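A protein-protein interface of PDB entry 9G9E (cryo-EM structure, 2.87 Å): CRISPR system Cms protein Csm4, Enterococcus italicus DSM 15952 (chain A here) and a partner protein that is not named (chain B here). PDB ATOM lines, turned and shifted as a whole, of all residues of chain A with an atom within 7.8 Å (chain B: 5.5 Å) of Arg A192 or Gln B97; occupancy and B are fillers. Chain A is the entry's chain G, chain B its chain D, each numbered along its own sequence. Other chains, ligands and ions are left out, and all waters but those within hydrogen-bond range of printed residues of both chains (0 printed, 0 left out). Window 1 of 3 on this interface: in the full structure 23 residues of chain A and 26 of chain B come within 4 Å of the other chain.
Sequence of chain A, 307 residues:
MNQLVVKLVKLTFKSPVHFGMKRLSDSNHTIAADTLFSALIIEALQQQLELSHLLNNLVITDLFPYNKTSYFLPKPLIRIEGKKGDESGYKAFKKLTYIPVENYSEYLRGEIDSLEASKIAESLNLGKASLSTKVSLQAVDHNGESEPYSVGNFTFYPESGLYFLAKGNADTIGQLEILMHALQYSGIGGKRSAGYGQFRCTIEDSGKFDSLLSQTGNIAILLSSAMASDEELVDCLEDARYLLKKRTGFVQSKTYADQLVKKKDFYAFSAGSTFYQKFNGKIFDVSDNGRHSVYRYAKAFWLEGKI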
ATOM      1  N   SER A  15       2.593 -31.856  -4.710  1.00  0.00           N
ATOM      2  CA  SER A  15       2.867 -30.889  -3.663  1.00  0.00           C
ATOM      3  C   SER A  15       1.625 -30.663  -2.817  1.00  0.00           C
ATOM      4  O   SER A  15       0.507 -30.993  -3.224  1.00  0.00           O
ATOM      5  CB  SER A  15       3.342 -29.573  -4.286  1.00  0.00           C
ATOM      6  OG  SER A  15       2.524 -29.204  -5.383  1.00  0.00           O
ATOM      7  N   PRO A  16       1.781 -30.109  -1.613  1.00  0.00           N
ATOM      8  CA  PRO A  16       0.601 -29.771  -0.809  1.00  0.00           C
ATOM      9  C   PRO A  16      -0.249 -28.718  -1.502  1.00  0.00           C
ATOM     10  O   PRO A  16       0.232 -27.948  -2.335  1.00  0.00           O
ATOM     11  CB  PRO A  16       1.198 -29.242   0.501  1.00  0.00           C
ATOM     12  CG  PRO A  16       2.610 -28.888   0.170  1.00  0.00           C
ATOM     13  CD  PRO A  16       3.031 -29.865  -0.876  1.00  0.00           C
ATOM     14  N   HIS A  18      -3.321 -25.625  -1.196  1.00  0.00           N
ATOM     15  CA  HIS A  18      -3.897 -24.590  -0.344  1.00  0.00           C
ATOM     16  C   HIS A  18      -5.316 -24.310  -0.823  1.00  0.00           C
ATOM     17  O   HIS A  18      -5.534 -23.452  -1.682  1.00  0.00           O
ATOM     18  CB  HIS A  18      -3.046 -23.326  -0.359  1.00  0.00           C
ATOM     19  CG  HIS A  18      -3.705 -22.156   0.302  1.00  0.00           C
ATOM     20  ND1 HIS A  18      -4.110 -22.177   1.617  1.00  0.00           N
ATOM     21  CD2 HIS A  18      -4.032 -20.932  -0.173  1.00  0.00           C
ATOM     22  CE1 HIS A  18      -4.663 -21.019   1.925  1.00  0.00           C
ATOM     23  NE2 HIS A  18      -4.624 -20.244   0.858  1.00  0.00           N
ATOM     24  N   ALA A  39     -11.859 -23.099 -12.376  1.00  0.00           N
ATOM     25  CA  ALA A  39     -10.553 -23.487 -12.898  1.00  0.00           C
ATOM     26  C   ALA A  39     -10.664 -24.024 -14.319  1.00  0.00           C
ATOM     27  O   ALA A  39      -9.824 -23.722 -15.174  1.00  0.00           O
ATOM     28  CB  ALA A  39      -9.907 -24.524 -11.979  1.00  0.00           C
ATOM     29  N   ILE A  42     -11.232 -21.086 -16.672  1.00  0.00           N
ATOM     30  CA  ILE A  42      -9.969 -20.376 -16.859  1.00  0.00           C
ATOM     31  C   ILE A  42      -9.062 -21.149 -17.808  1.00  0.00           C
ATOM     32  O   ILE A  42      -8.407 -20.565 -18.681  1.00  0.00           O
ATOM     33  CB  ILE A  42      -9.293 -20.127 -15.498  1.00  0.00           C
ATOM     34  CG1 ILE A  42     -10.065 -19.072 -14.704  1.00  0.00           C
ATOM     35  CG2 ILE A  42      -7.847 -19.698 -15.684  1.00  0.00           C
ATOM     36  CD1 ILE A  42      -9.528 -18.843 -13.311  1.00  0.00           C
ATOM     37  N   GLU A  43      -9.012 -22.474 -17.655  1.00  0.00           N
ATOM     38  CA  GLU A  43      -8.202 -23.300 -18.544  1.00  0.00           C
ATOM     39  C   GLU A  43      -8.702 -23.229 -19.981  1.00  0.00           C
ATOM     40  O   GLU A  43      -7.902 -23.158 -20.922  1.00  0.00           O
ATOM     41  CB  GLU A  43      -8.197 -24.745 -18.052  1.00  0.00           C
ATOM     42  CG  GLU A  43      -6.919 -25.477 -18.365  1.00  0.00           C
ATOM     43  CD  GLU A  43      -5.730 -24.853 -17.675  1.00  0.00           C
ATOM     44  OE1 GLU A  43      -5.884 -24.406 -16.521  1.00  0.00           O
ATOM     45  OE2 GLU A  43      -4.648 -24.795 -18.292  1.00  0.00           O
ATOM     46  N   GLN A  46      -7.630 -20.016 -21.416  1.00  0.00           N
ATOM     47  CA  GLN A  46      -6.201 -20.060 -21.707  1.00  0.00           C
ATOM     48  C   GLN A  46      -5.932 -20.788 -23.020  1.00  0.00           C
ATOM     49  O   GLN A  46      -5.123 -20.341 -23.839  1.00  0.00           O
ATOM     50  CB  GLN A  46      -5.452 -20.733 -20.557  1.00  0.00           C
ATOM     51  CG  GLN A  46      -5.226 -19.842 -19.350  1.00  0.00           C
ATOM     52  CD  GLN A  46      -4.448 -20.539 -18.251  1.00  0.00           C
ATOM     53  OE1 GLN A  46      -4.068 -21.701 -18.387  1.00  0.00           O
ATOM     54  NE2 GLN A  46      -4.212 -19.832 -17.152  1.00  0.00           N
ATOM     55  N   ALA A 182      -4.416 -30.037 -19.086  1.00  0.00           N
ATOM     56  CA  ALA A 182      -3.776 -28.743 -18.859  1.00  0.00           C
ATOM     57  C   ALA A 182      -3.840 -28.328 -17.389  1.00  0.00           C
ATOM     58  O   ALA A 182      -2.926 -27.660 -16.889  1.00  0.00           O
ATOM     59  CB  ALA A 182      -4.418 -27.679 -19.747  1.00  0.00           C
ATOM     60  N   LEU A 183      -4.906 -28.715 -16.686  1.00  0.00           N
ATOM     61  CA  LEU A 183      -5.063 -28.335 -15.288  1.00  0.00           C
ATOM     62  C   LEU A 183      -4.061 -29.046 -14.390  1.00  0.00           C
ATOM     63  O   LEU A 183      -3.761 -28.552 -13.297  1.00  0.00           O
ATOM     64  CB  LEU A 183      -6.491 -28.627 -14.826  1.00  0.00           C
ATOM     65  CG  LEU A 183      -7.063 -27.753 -13.708  1.00  0.00           C
ATOM     66  CD1 LEU A 183      -6.876 -26.279 -14.020  1.00  0.00           C
ATOM     67  CD2 LEU A 183      -8.532 -28.072 -13.486  1.00  0.00           C
ATOM     68  N   GLN A 184      -3.562 -30.213 -14.810  1.00  0.00           N
ATOM     69  CA  GLN A 184      -2.499 -30.863 -14.044  1.00  0.00           C
ATOM     70  C   GLN A 184      -1.331 -29.915 -13.814  1.00  0.00           C
ATOM     71  O   GLN A 184      -0.751 -29.879 -12.723  1.00  0.00           O
ATOM     72  CB  GLN A 184      -1.995 -32.129 -14.743  1.00  0.00           C
ATOM     73  CG  GLN A 184      -3.029 -32.946 -15.466  1.00  0.00           C
ATOM     74  CD  GLN A 184      -2.482 -34.275 -15.942  1.00  0.00           C
ATOM     75  OE1 GLN A 184      -1.328 -34.612 -15.683  1.00  0.00           O
ATOM     76  NE2 GLN A 184      -3.311 -35.040 -16.642  1.00  0.00           N
ATOM     77  N   TYR A 185      -0.977 -29.133 -14.834  1.00  0.00           N
ATOM     78  CA  TYR A 185       0.151 -28.220 -14.757  1.00  0.00           C
ATOM     79  C   TYR A 185      -0.246 -26.793 -14.413  1.00  0.00           C
ATOM     80  O   TYR A 185       0.612 -26.020 -13.974  1.00  0.00           O
ATOM     81  CB  TYR A 185       0.922 -28.234 -16.080  1.00  0.00           C
ATOM     82  CG  TYR A 185       1.212 -29.633 -16.573  1.00  0.00           C
ATOM     83  CD1 TYR A 185       2.216 -30.397 -15.996  1.00  0.00           C
ATOM     84  CD2 TYR A 185       0.468 -30.197 -17.599  1.00  0.00           C
ATOM     85  CE1 TYR A 185       2.482 -31.677 -16.436  1.00  0.00           C
ATOM     86  CE2 TYR A 185       0.726 -31.477 -18.047  1.00  0.00           C
ATOM     87  CZ  TYR A 185       1.734 -32.213 -17.462  1.00  0.00           C
ATOM     88  OH  TYR A 185       1.995 -33.489 -17.904  1.00  0.00           O
ATOM     89  N   SER A 186      -1.514 -26.419 -14.604  1.00  0.00           N
ATOM     90  CA  SER A 186      -1.967 -25.131 -14.085  1.00  0.00           C
ATOM     91  C   SER A 186      -2.071 -25.153 -12.565  1.00  0.00           C
ATOM     92  O   SER A 186      -1.691 -24.185 -11.896  1.00  0.00           O
ATOM     93  CB  SER A 186      -3.307 -24.745 -14.703  1.00  0.00           C
ATOM     94  OG  SER A 186      -3.133 -24.217 -16.004  1.00  0.00           O
ATOM     95  N   GLY A 187      -2.578 -26.240 -12.005  1.00  0.00           N
ATOM     96  CA  GLY A 187      -2.769 -26.331 -10.566  1.00  0.00           C
ATOM     97  C   GLY A 187      -4.134 -25.835 -10.136  1.00  0.00           C
ATOM     98  O   GLY A 187      -4.793 -25.054 -10.821  1.00  0.00           O
ATOM     99  N   ILE A 188      -4.570 -26.310  -8.973  1.00  0.00           N
ATOM    100  CA  ILE A 188      -5.849 -25.921  -8.393  1.00  0.00           C
ATOM    101  C   ILE A 188      -5.617 -25.463  -6.961  1.00  0.00           C
ATOM    102  O   ILE A 188      -4.793 -26.036  -6.240  1.00  0.00           O
ATOM    103  CB  ILE A 188      -6.879 -27.069  -8.437  1.00  0.00           C
ATOM    104  CG1 ILE A 188      -6.304 -28.337  -7.808  1.00  0.00           C
ATOM    105  CG2 ILE A 188      -7.326 -27.331  -9.866  1.00  0.00           C
ATOM    106  CD1 ILE A 188      -7.258 -29.509  -7.826  1.00  0.00           C
ATOM    107  N   GLY A 189      -6.339 -24.422  -6.556  1.00  0.00           N
ATOM    108  CA  GLY A 189      -6.273 -23.960  -5.186  1.00  0.00           C
ATOM    109  C   GLY A 189      -5.735 -22.556  -5.018  1.00  0.00           C
ATOM    110  O   GLY A 189      -6.147 -21.630  -5.721  1.00  0.00           O
ATOM    111  N   GLY A 190      -4.800 -22.395  -4.089  1.00  0.00           N
ATOM    112  CA  GLY A 190      -4.327 -21.086  -3.689  1.00  0.00           C
ATOM    113  C   GLY A 190      -3.056 -20.670  -4.391  1.00  0.00           C
ATOM    114  O   GLY A 190      -3.093 -20.259  -5.552  1.00  0.00           O
ATOM    115  N   LYS A 191      -1.925 -20.761  -3.694  1.00  0.00           N
ATOM    116  CA  LYS A 191      -0.644 -20.320  -4.233  1.00  0.00           C
ATOM    117  C   LYS A 191      -0.102 -21.308  -5.259  1.00  0.00           C
ATOM    118  O   LYS A 191       0.888 -21.999  -5.000  1.00  0.00           O
ATOM    119  CB  LYS A 191       0.364 -20.127  -3.101  1.00  0.00           C
ATOM    120  CG  LYS A 191      -0.225 -19.528  -1.835  1.00  0.00           C
ATOM    121  CD  LYS A 191      -0.484 -18.041  -1.996  1.00  0.00           C
ATOM    122  CE  LYS A 191       0.787 -17.239  -1.778  1.00  0.00           C
ATOM    123  NZ  LYS A 191       0.552 -15.777  -1.914  1.00  0.00           N
ATOM    124  N   ARG A 192      -0.746 -21.379  -6.425  1.00  0.00           N
ATOM    125  CA  ARG A 192      -0.289 -22.279  -7.479  1.00  0.00           C
ATOM    126  C   ARG A 192       1.073 -21.857  -8.015  1.00  0.00           C
ATOM    127  O   ARG A 192       1.919 -22.707  -8.316  1.00  0.00           O
ATOM    128  CB  ARG A 192      -1.322 -22.330  -8.602  1.00  0.00           C
ATOM    129  CG  ARG A 192      -2.755 -22.317  -8.110  1.00  0.00           C
ATOM    130  CD  ARG A 192      -3.738 -22.266  -9.262  1.00  0.00           C
ATOM    131  NE  ARG A 192      -3.839 -20.932  -9.840  1.00  0.00           N
ATOM    132  CZ  ARG A 192      -3.516 -20.628 -11.089  1.00  0.00           C
ATOM    133  NH1 ARG A 192      -3.053 -21.543 -11.924  1.00  0.00           N
ATOM    134  NH2 ARG A 192      -3.665 -19.376 -11.512  1.00  0.00           N
ATOM    135  N   SER A 193       1.300 -20.552  -8.147  1.00  0.00           N
ATOM    136  CA  SER A 193       2.578 -20.043  -8.621  1.00  0.00           C
ATOM    137  C   SER A 193       3.656 -20.050  -7.546  1.00  0.00           C
ATOM    138  O   SER A 193       4.829 -19.830  -7.869  1.00  0.00           O
ATOM    139  CB  SER A 193       2.406 -18.625  -9.165  1.00  0.00           C
ATOM    140  OG  SER A 193       1.299 -18.553 -10.048  1.00  0.00           O
ATOM    141  N   ALA A 194       3.296 -20.294  -6.285  1.00  0.00           N
ATOM    142  CA  ALA A 194       4.250 -20.311  -5.183  1.00  0.00           C
ATOM    143  C   ALA A 194       4.488 -21.722  -4.650  1.00  0.00           C
ATOM    144  O   ALA A 194       4.961 -21.894  -3.525  1.00  0.00           O
ATOM    145  CB  ALA A 194       3.785 -19.389  -4.059  1.00  0.00           C
ATOM    146  N   GLY A 195       4.164 -22.738  -5.442  1.00  0.00           N
ATOM    147  CA  GLY A 195       4.478 -24.104  -5.102  1.00  0.00           C
ATOM    148  C   GLY A 195       3.371 -24.921  -4.476  1.00  0.00           C
ATOM    149  O   GLY A 195       3.655 -25.723  -3.579  1.00  0.00           O
ATOM    150  N   TYR A 196       2.126 -24.750  -4.911  1.00  0.00           N
ATOM    151  CA  TYR A 196       1.007 -25.508  -4.375  1.00  0.00           C
ATOM    152  C   TYR A 196       0.064 -25.903  -5.503  1.00  0.00           C
ATOM    153  O   TYR A 196       0.054 -25.295  -6.575  1.00  0.00           O
ATOM    154  CB  TYR A 196       0.241 -24.706  -3.311  1.00  0.00           C
ATOM    155  CG  TYR A 196       1.036 -24.419  -2.057  1.00  0.00           C
ATOM    156  CD1 TYR A 196       1.297 -25.418  -1.133  1.00  0.00           C
ATOM    157  CD2 TYR A 196       1.521 -23.147  -1.796  1.00  0.00           C
ATOM    158  CE1 TYR A 196       2.019 -25.162   0.013  1.00  0.00           C
ATOM    159  CE2 TYR A 196       2.244 -22.880  -0.651  1.00  0.00           C
ATOM    160  CZ  TYR A 196       2.491 -23.892   0.249  1.00  0.00           C
ATOM    161  OH  TYR A 196       3.211 -23.633   1.391  1.00  0.00           O
ATOM    162  N   GLY A 197      -0.724 -26.946  -5.252  1.00  0.00           N
ATOM    163  CA  GLY A 197      -1.807 -27.318  -6.137  1.00  0.00           C
ATOM    164  C   GLY A 197      -1.431 -28.155  -7.339  1.00  0.00           C
ATOM    165  O   GLY A 197      -2.319 -28.494  -8.131  1.00  0.00           O
ATOM    166  N   GLN A 198      -0.158 -28.501  -7.511  1.00  0.00           N
ATOM    167  CA  GLN A 198       0.236 -29.328  -8.643  1.00  0.00           C
ATOM    168  C   GLN A 198      -0.231 -30.763  -8.440  1.00  0.00           C
ATOM    169  O   GLN A 198      -0.085 -31.334  -7.356  1.00  0.00           O
ATOM    170  CB  GLN A 198       1.752 -29.286  -8.831  1.00  0.00           C
ATOM    171  CG  GLN A 198       2.267 -27.985  -9.423  1.00  0.00           C
ATOM    172  CD  GLN A 198       1.986 -27.867 -10.908  1.00  0.00           C
ATOM    173  OE1 GLN A 198       1.798 -28.869 -11.598  1.00  0.00           O
ATOM    174  NE2 GLN A 198       1.957 -26.638 -11.408  1.00  0.00           N
ATOM    175  N   GLN A 252     -10.566 -13.780  -9.913  1.00  0.00           N
ATOM    176  CA  GLN A 252      -9.217 -14.047 -10.412  1.00  0.00           C
ATOM    177  C   GLN A 252      -9.240 -13.877 -11.925  1.00  0.00           C
ATOM    178  O   GLN A 252      -9.559 -14.801 -12.674  1.00  0.00           O
ATOM    179  CB  GLN A 252      -8.754 -15.440 -10.008  1.00  0.00           C
ATOM    180  CG  GLN A 252      -7.410 -15.844 -10.599  1.00  0.00           C
ATOM    181  CD  GLN A 252      -6.942 -17.202 -10.119  1.00  0.00           C
ATOM    182  OE1 GLN A 252      -7.115 -17.559  -8.955  1.00  0.00           O
ATOM    183  NE2 GLN A 252      -6.337 -17.968 -11.019  1.00  0.00           N
ATOM    184  N   LYS A 254      -7.281 -11.137 -15.146  1.00  0.00           N
ATOM    185  CA  LYS A 254      -6.416 -10.020 -15.498  1.00  0.00           C
ATOM    186  C   LYS A 254      -7.119  -8.965 -16.341  1.00  0.00           C
ATOM    187  O   LYS A 254      -6.519  -7.923 -16.624  1.00  0.00           O
ATOM    188  CB  LYS A 254      -5.164 -10.509 -16.249  1.00  0.00           C
ATOM    189  CG  LYS A 254      -4.330 -11.650 -15.623  1.00  0.00           C
ATOM    190  CD  LYS A 254      -4.570 -11.892 -14.135  1.00  0.00           C
ATOM    191  CE  LYS A 254      -4.046 -13.254 -13.706  1.00  0.00           C
ATOM    192  NZ  LYS A 254      -4.114 -13.448 -12.231  1.00  0.00           N
ATOM    193  N   LYS B   4       2.920 -24.813 -22.021  1.00  0.00           N
ATOM    194  CA  LYS B   4       3.552 -24.909 -20.716  1.00  0.00           C
ATOM    195  C   LYS B   4       4.763 -25.815 -20.848  1.00  0.00           C
ATOM    196  O   LYS B   4       4.645 -26.940 -21.347  1.00  0.00           O
ATOM    197  CB  LYS B   4       2.588 -25.464 -19.666  1.00  0.00           C
ATOM    198  CG  LYS B   4       1.756 -24.410 -18.974  1.00  0.00           C
ATOM    199  CD  LYS B   4       0.631 -25.059 -18.197  1.00  0.00           C
ATOM    200  CE  LYS B   4      -0.602 -25.186 -19.067  1.00  0.00           C
ATOM    201  NZ  LYS B   4      -1.839 -25.285 -18.264  1.00  0.00           N
ATOM    202  N   SER B  94       1.546 -14.764 -13.178  1.00  0.00           N
ATOM    203  CA  SER B  94       2.876 -15.313 -12.948  1.00  0.00           C
ATOM    204  C   SER B  94       3.178 -16.392 -13.981  1.00  0.00           C
ATOM    205  O   SER B  94       2.485 -17.412 -14.046  1.00  0.00           O
ATOM    206  CB  SER B  94       2.976 -15.877 -11.535  1.00  0.00           C
ATOM    207  OG  SER B  94       4.206 -16.550 -11.340  1.00  0.00           O
ATOM    208  N   ARG B  95       4.213 -16.163 -14.791  1.00  0.00           N
ATOM    209  CA  ARG B  95       4.598 -17.140 -15.802  1.00  0.00           C
ATOM    210  C   ARG B  95       5.338 -18.326 -15.200  1.00  0.00           C
ATOM    211  O   ARG B  95       5.242 -19.441 -15.724  1.00  0.00           O
ATOM    212  CB  ARG B  95       5.456 -16.473 -16.878  1.00  0.00           C
ATOM    213  CG  ARG B  95       4.647 -15.683 -17.888  1.00  0.00           C
ATOM    214  CD  ARG B  95       5.523 -14.835 -18.791  1.00  0.00           C
ATOM    215  NE  ARG B  95       4.718 -14.011 -19.686  1.00  0.00           N
ATOM    216  CZ  ARG B  95       5.208 -13.087 -20.502  1.00  0.00           C
ATOM    217  NH1 ARG B  95       6.505 -12.838 -20.565  1.00  0.00           N
ATOM    218  NH2 ARG B  95       4.375 -12.397 -21.274  1.00  0.00           N
ATOM    219  N   LEU B  96       6.068 -18.117 -14.111  1.00  0.00           N
ATOM    220  CA  LEU B  96       6.839 -19.173 -13.467  1.00  0.00           C
ATOM    221  C   LEU B  96       6.067 -19.711 -12.271  1.00  0.00           C
ATOM    222  O   LEU B  96       5.751 -18.960 -11.342  1.00  0.00           O
ATOM    223  CB  LEU B  96       8.207 -18.657 -13.023  1.00  0.00           C
ATOM    224  CG  LEU B  96       9.307 -18.580 -14.077  1.00  0.00           C
ATOM    225  CD1 LEU B  96      10.551 -17.942 -13.485  1.00  0.00           C
ATOM    226  CD2 LEU B  96       9.613 -19.962 -14.625  1.00  0.00           C
ATOM    227  N   GLN B  97       5.768 -21.007 -12.294  1.00  0.00           N
ATOM    228  CA  GLN B  97       5.224 -21.719 -11.145  1.00  0.00           C
ATOM    229  C   GLN B  97       6.305 -22.672 -10.654  1.00  0.00           C
ATOM    230  O   GLN B  97       6.571 -23.696 -11.291  1.00  0.00           O
ATOM    231  CB  GLN B  97       3.947 -22.472 -11.508  1.00  0.00           C
ATOM    232  CG  GLN B  97       3.021 -21.720 -12.442  1.00  0.00           C
ATOM    233  CD  GLN B  97       1.699 -22.431 -12.637  1.00  0.00           C
ATOM    234  OE1 GLN B  97       1.146 -23.003 -11.699  1.00  0.00           O
ATOM    235  NE2 GLN B  97       1.187 -22.404 -13.861  1.00  0.00           N
ATOM    236  N   ILE B  98       6.933 -22.328  -9.537  1.00  0.00           N
ATOM    237  CA  ILE B  98       8.029 -23.107  -8.978  1.00  0.00           C
ATOM    238  C   ILE B  98       7.469 -23.920  -7.820  1.00  0.00           C
ATOM    239  O   ILE B  98       7.098 -23.366  -6.780  1.00  0.00           O
ATOM    240  CB  ILE B  98       9.188 -22.208  -8.527  1.00  0.00           C
ATOM    241  CG1 ILE B  98       9.672 -21.345  -9.694  1.00  0.00           C
ATOM    242  CG2 ILE B  98      10.326 -23.046  -7.971  1.00  0.00           C
ATOM    243  CD1 ILE B  98      10.672 -20.287  -9.301  1.00  0.00           C
ATOM    244  N   SER B  99       7.406 -25.235  -8.000  1.00  0.00           N
ATOM    245  CA  SER B  99       6.870 -26.115  -6.977  1.00  0.00           C
ATOM    246  C   SER B  99       7.913 -26.376  -5.895  1.00  0.00           C
ATOM    247  O   SER B  99       9.104 -26.100  -6.061  1.00  0.00           O
ATOM    248  CB  SER B  99       6.409 -27.436  -7.591  1.00  0.00           C
ATOM    249  OG  SER B  99       5.634 -27.213  -8.757  1.00  0.00           O
ATOM    250  N   HIS B 151      10.843 -28.896  -9.610  1.00  0.00           N
ATOM    251  CA  HIS B 151       9.917 -28.945 -10.735  1.00  0.00           C
ATOM    252  C   HIS B 151       9.373 -27.544 -10.966  1.00  0.00           C
ATOM    253  O   HIS B 151       8.830 -26.931 -10.042  1.00  0.00           O
ATOM    254  CB  HIS B 151       8.782 -29.935 -10.452  1.00  0.00           C
ATOM    255  CG  HIS B 151       7.629 -29.833 -11.399  1.00  0.00           C
ATOM    256  ND1 HIS B 151       6.408 -29.314 -11.026  1.00  0.00           N
ATOM    257  CD2 HIS B 151       7.503 -30.193 -12.696  1.00  0.00           C
ATOM    258  CE1 HIS B 151       5.581 -29.353 -12.055  1.00  0.00           C
ATOM    259  NE2 HIS B 151       6.221 -29.882 -13.082  1.00  0.00           N
ATOM    260  N   ILE B 152       9.518 -27.039 -12.189  1.00  0.00           N
ATOM    261  CA  ILE B 152       9.103 -25.688 -12.544  1.00  0.00           C
ATOM    262  C   ILE B 152       8.240 -25.759 -13.796  1.00  0.00           C
ATOM    263  O   ILE B 152       8.511 -26.550 -14.703  1.00  0.00           O
ATOM    264  CB  ILE B 152      10.321 -24.763 -12.769  1.00  0.00           C
ATOM    265  CG1 ILE B 152      11.154 -24.652 -11.492  1.00  0.00           C
ATOM    266  CG2 ILE B 152       9.883 -23.382 -13.226  1.00  0.00           C
ATOM    267  CD1 ILE B 152      12.341 -23.725 -11.617  1.00  0.00           C
ATOM    268  N   ILE B 153       7.187 -24.947 -13.837  1.00  0.00           N
ATOM    269  CA  ILE B 153       6.324 -24.835 -15.008  1.00  0.00           C
ATOM    270  C   ILE B 153       6.410 -23.404 -15.517  1.00  0.00           C
ATOM    271  O   ILE B 153       6.119 -22.456 -14.777  1.00  0.00           O
ATOM    272  CB  ILE B 153       4.870 -25.215 -14.689  1.00  0.00           C
ATOM    273  CG1 ILE B 153       4.782 -26.678 -14.250  1.00  0.00           C
ATOM    274  CG2 ILE B 153       3.975 -24.956 -15.894  1.00  0.00           C
ATOM    275  CD1 ILE B 153       4.666 -27.659 -15.395  1.00  0.00           C
ATOM    276  N   TYR B 154       6.812 -23.244 -16.775  1.00  0.00           N
ATOM    277  CA  TYR B 154       6.824 -21.938 -17.421  1.00  0.00           C
ATOM    278  C   TYR B 154       5.622 -21.845 -18.352  1.00  0.00           C
ATOM    279  O   TYR B 154       5.445 -22.695 -19.231  1.00  0.00           O
ATOM    280  CB  TYR B 154       8.123 -21.700 -18.190  1.00  0.00           C
ATOM    281  CG  TYR B 154       8.109 -20.412 -18.985  1.00  0.00           C
ATOM    282  CD1 TYR B 154       8.472 -19.207 -18.398  1.00  0.00           C
ATOM    283  CD2 TYR B 154       7.726 -20.400 -20.320  1.00  0.00           C
ATOM    284  CE1 TYR B 154       8.453 -18.029 -19.117  1.00  0.00           C
ATOM    285  CE2 TYR B 154       7.703 -19.227 -21.045  1.00  0.00           C
ATOM    286  CZ  TYR B 154       8.069 -18.046 -20.442  1.00  0.00           C
ATOM    287  OH  TYR B 154       8.046 -16.880 -21.169  1.00  0.00           O
ATOM    288  N   ASN B 155       4.804 -20.815 -18.153  1.00  0.00           N
ATOM    289  CA  ASN B 155       3.601 -20.595 -18.945  1.00  0.00           C
ATOM    290  C   ASN B 155       3.914 -19.626 -20.078  1.00  0.00           C
ATOM    291  O   ASN B 155       4.362 -18.502 -19.830  1.00  0.00           O
ATOM    292  CB  ASN B 155       2.482 -20.040 -18.067  1.00  0.00           C
ATOM    293  CG  ASN B 155       2.145 -20.949 -16.905  1.00  0.00           C
ATOM    294  OD1 ASN B 155       2.774 -20.884 -15.850  1.00  0.00           O
ATOM    295  ND2 ASN B 155       1.134 -21.788 -17.085  1.00  0.00           N
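Lys B4 touches Tyr A185.
O of Tyr A185 touches NE2 of Gln B97, 3.7 Å away.
Ile B153 touches Tyr A185.
OG of Ser A193 touches CB of Ser B94, at 3.5 Å.
Leu B96 touches Ser A193.
Ser A193 touches Ile B98.
Ile B98 touches Ala A194 (O to C, 3.7 Å).
Gly A195 touches Ser B99 (CA to CA, 3.6 Å).
Gln A198 touches Gln B97 (NE2 to OE1, 3.7 Å).
CG of Gln A198 touches OG of Ser B99, 3.5 Å away.
Of chain A, only Tyr A185 (3.7 Å), Ser A186 (3.1 Å), Arg A192 (3.5 Å), Ser A193 (3.8 Å) and Gln A198 (3.7 Å) come within 4 Å of Gln B97.
Of the printed residues of chain B, Tyr A185 touches Lys B4, Gln B97 and Ile B153.
Of the printed residues of chain B, Ala A194 touches Ile B98.
Printed residues of chain B within 4 Å of Gly A195: Ile B98 and Ser B99.
The nearest residue of chain A that does not touch Gln B97 is Gly A187 (4.9 Å).
The nearest printed residue of chain B that does not touch Gln A198 is Ile B153 (4.01 Å).
NZ of Lys B4 lies within salt-bridge range of OE2 of Glu A43 (2.9 Å).
O of Ala A182 lies within hydrogen-bond range of NZ of Lys B4, 3.0 Å away.
OG of Ser A186 is in hydrogen-bond range of NZ of Lys B4 (2.8 Å).
The backbone carbonyl oxygen (O) of Ser A186 lies close to the side-chain amide oxygen (OE1) of Gln B97.
O of Arg A192 sits close to OE1 of Gln B97 (3.5 Å).
O of Ile B98 sits close to N of Gly A195, at 3.3 Å.
The backbone carbonyl oxygen of Leu B96 is in hydrogen-bond range of the side-chain hydroxyl of Ser B94 (2.9 Å).
The backbone carbonyl oxygen of Ile B153 sits at hydrogen-bond distance from the backbone NH of Gln B97 (2.9 Å).
The side-chain amide oxygen (OD1) of Asn B155 sits at hydrogen-bond distance from the side-chain amide nitrogen (NE2) of Gln B97.
The side-chain hydroxyl (OG) of Ser A15 is in hydrogen-bond range of the backbone NH (N) of Gln A198.
The side-chain carboxylate (OE2) of Glu A43 is in hydrogen-bond range of the side-chain hydroxyl (OG) of Ser A186 (2.8 Å).
The backbone carbonyl oxygen (O) of Tyr A185 sits at hydrogen-bond distance from the side-chain amide nitrogen (NE2) of Gln A198 (3.0 Å).
Hydrophobic or aromatic side chains of chain B within 4 Å of the printed part of chain A: His B151 and Ile B153.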
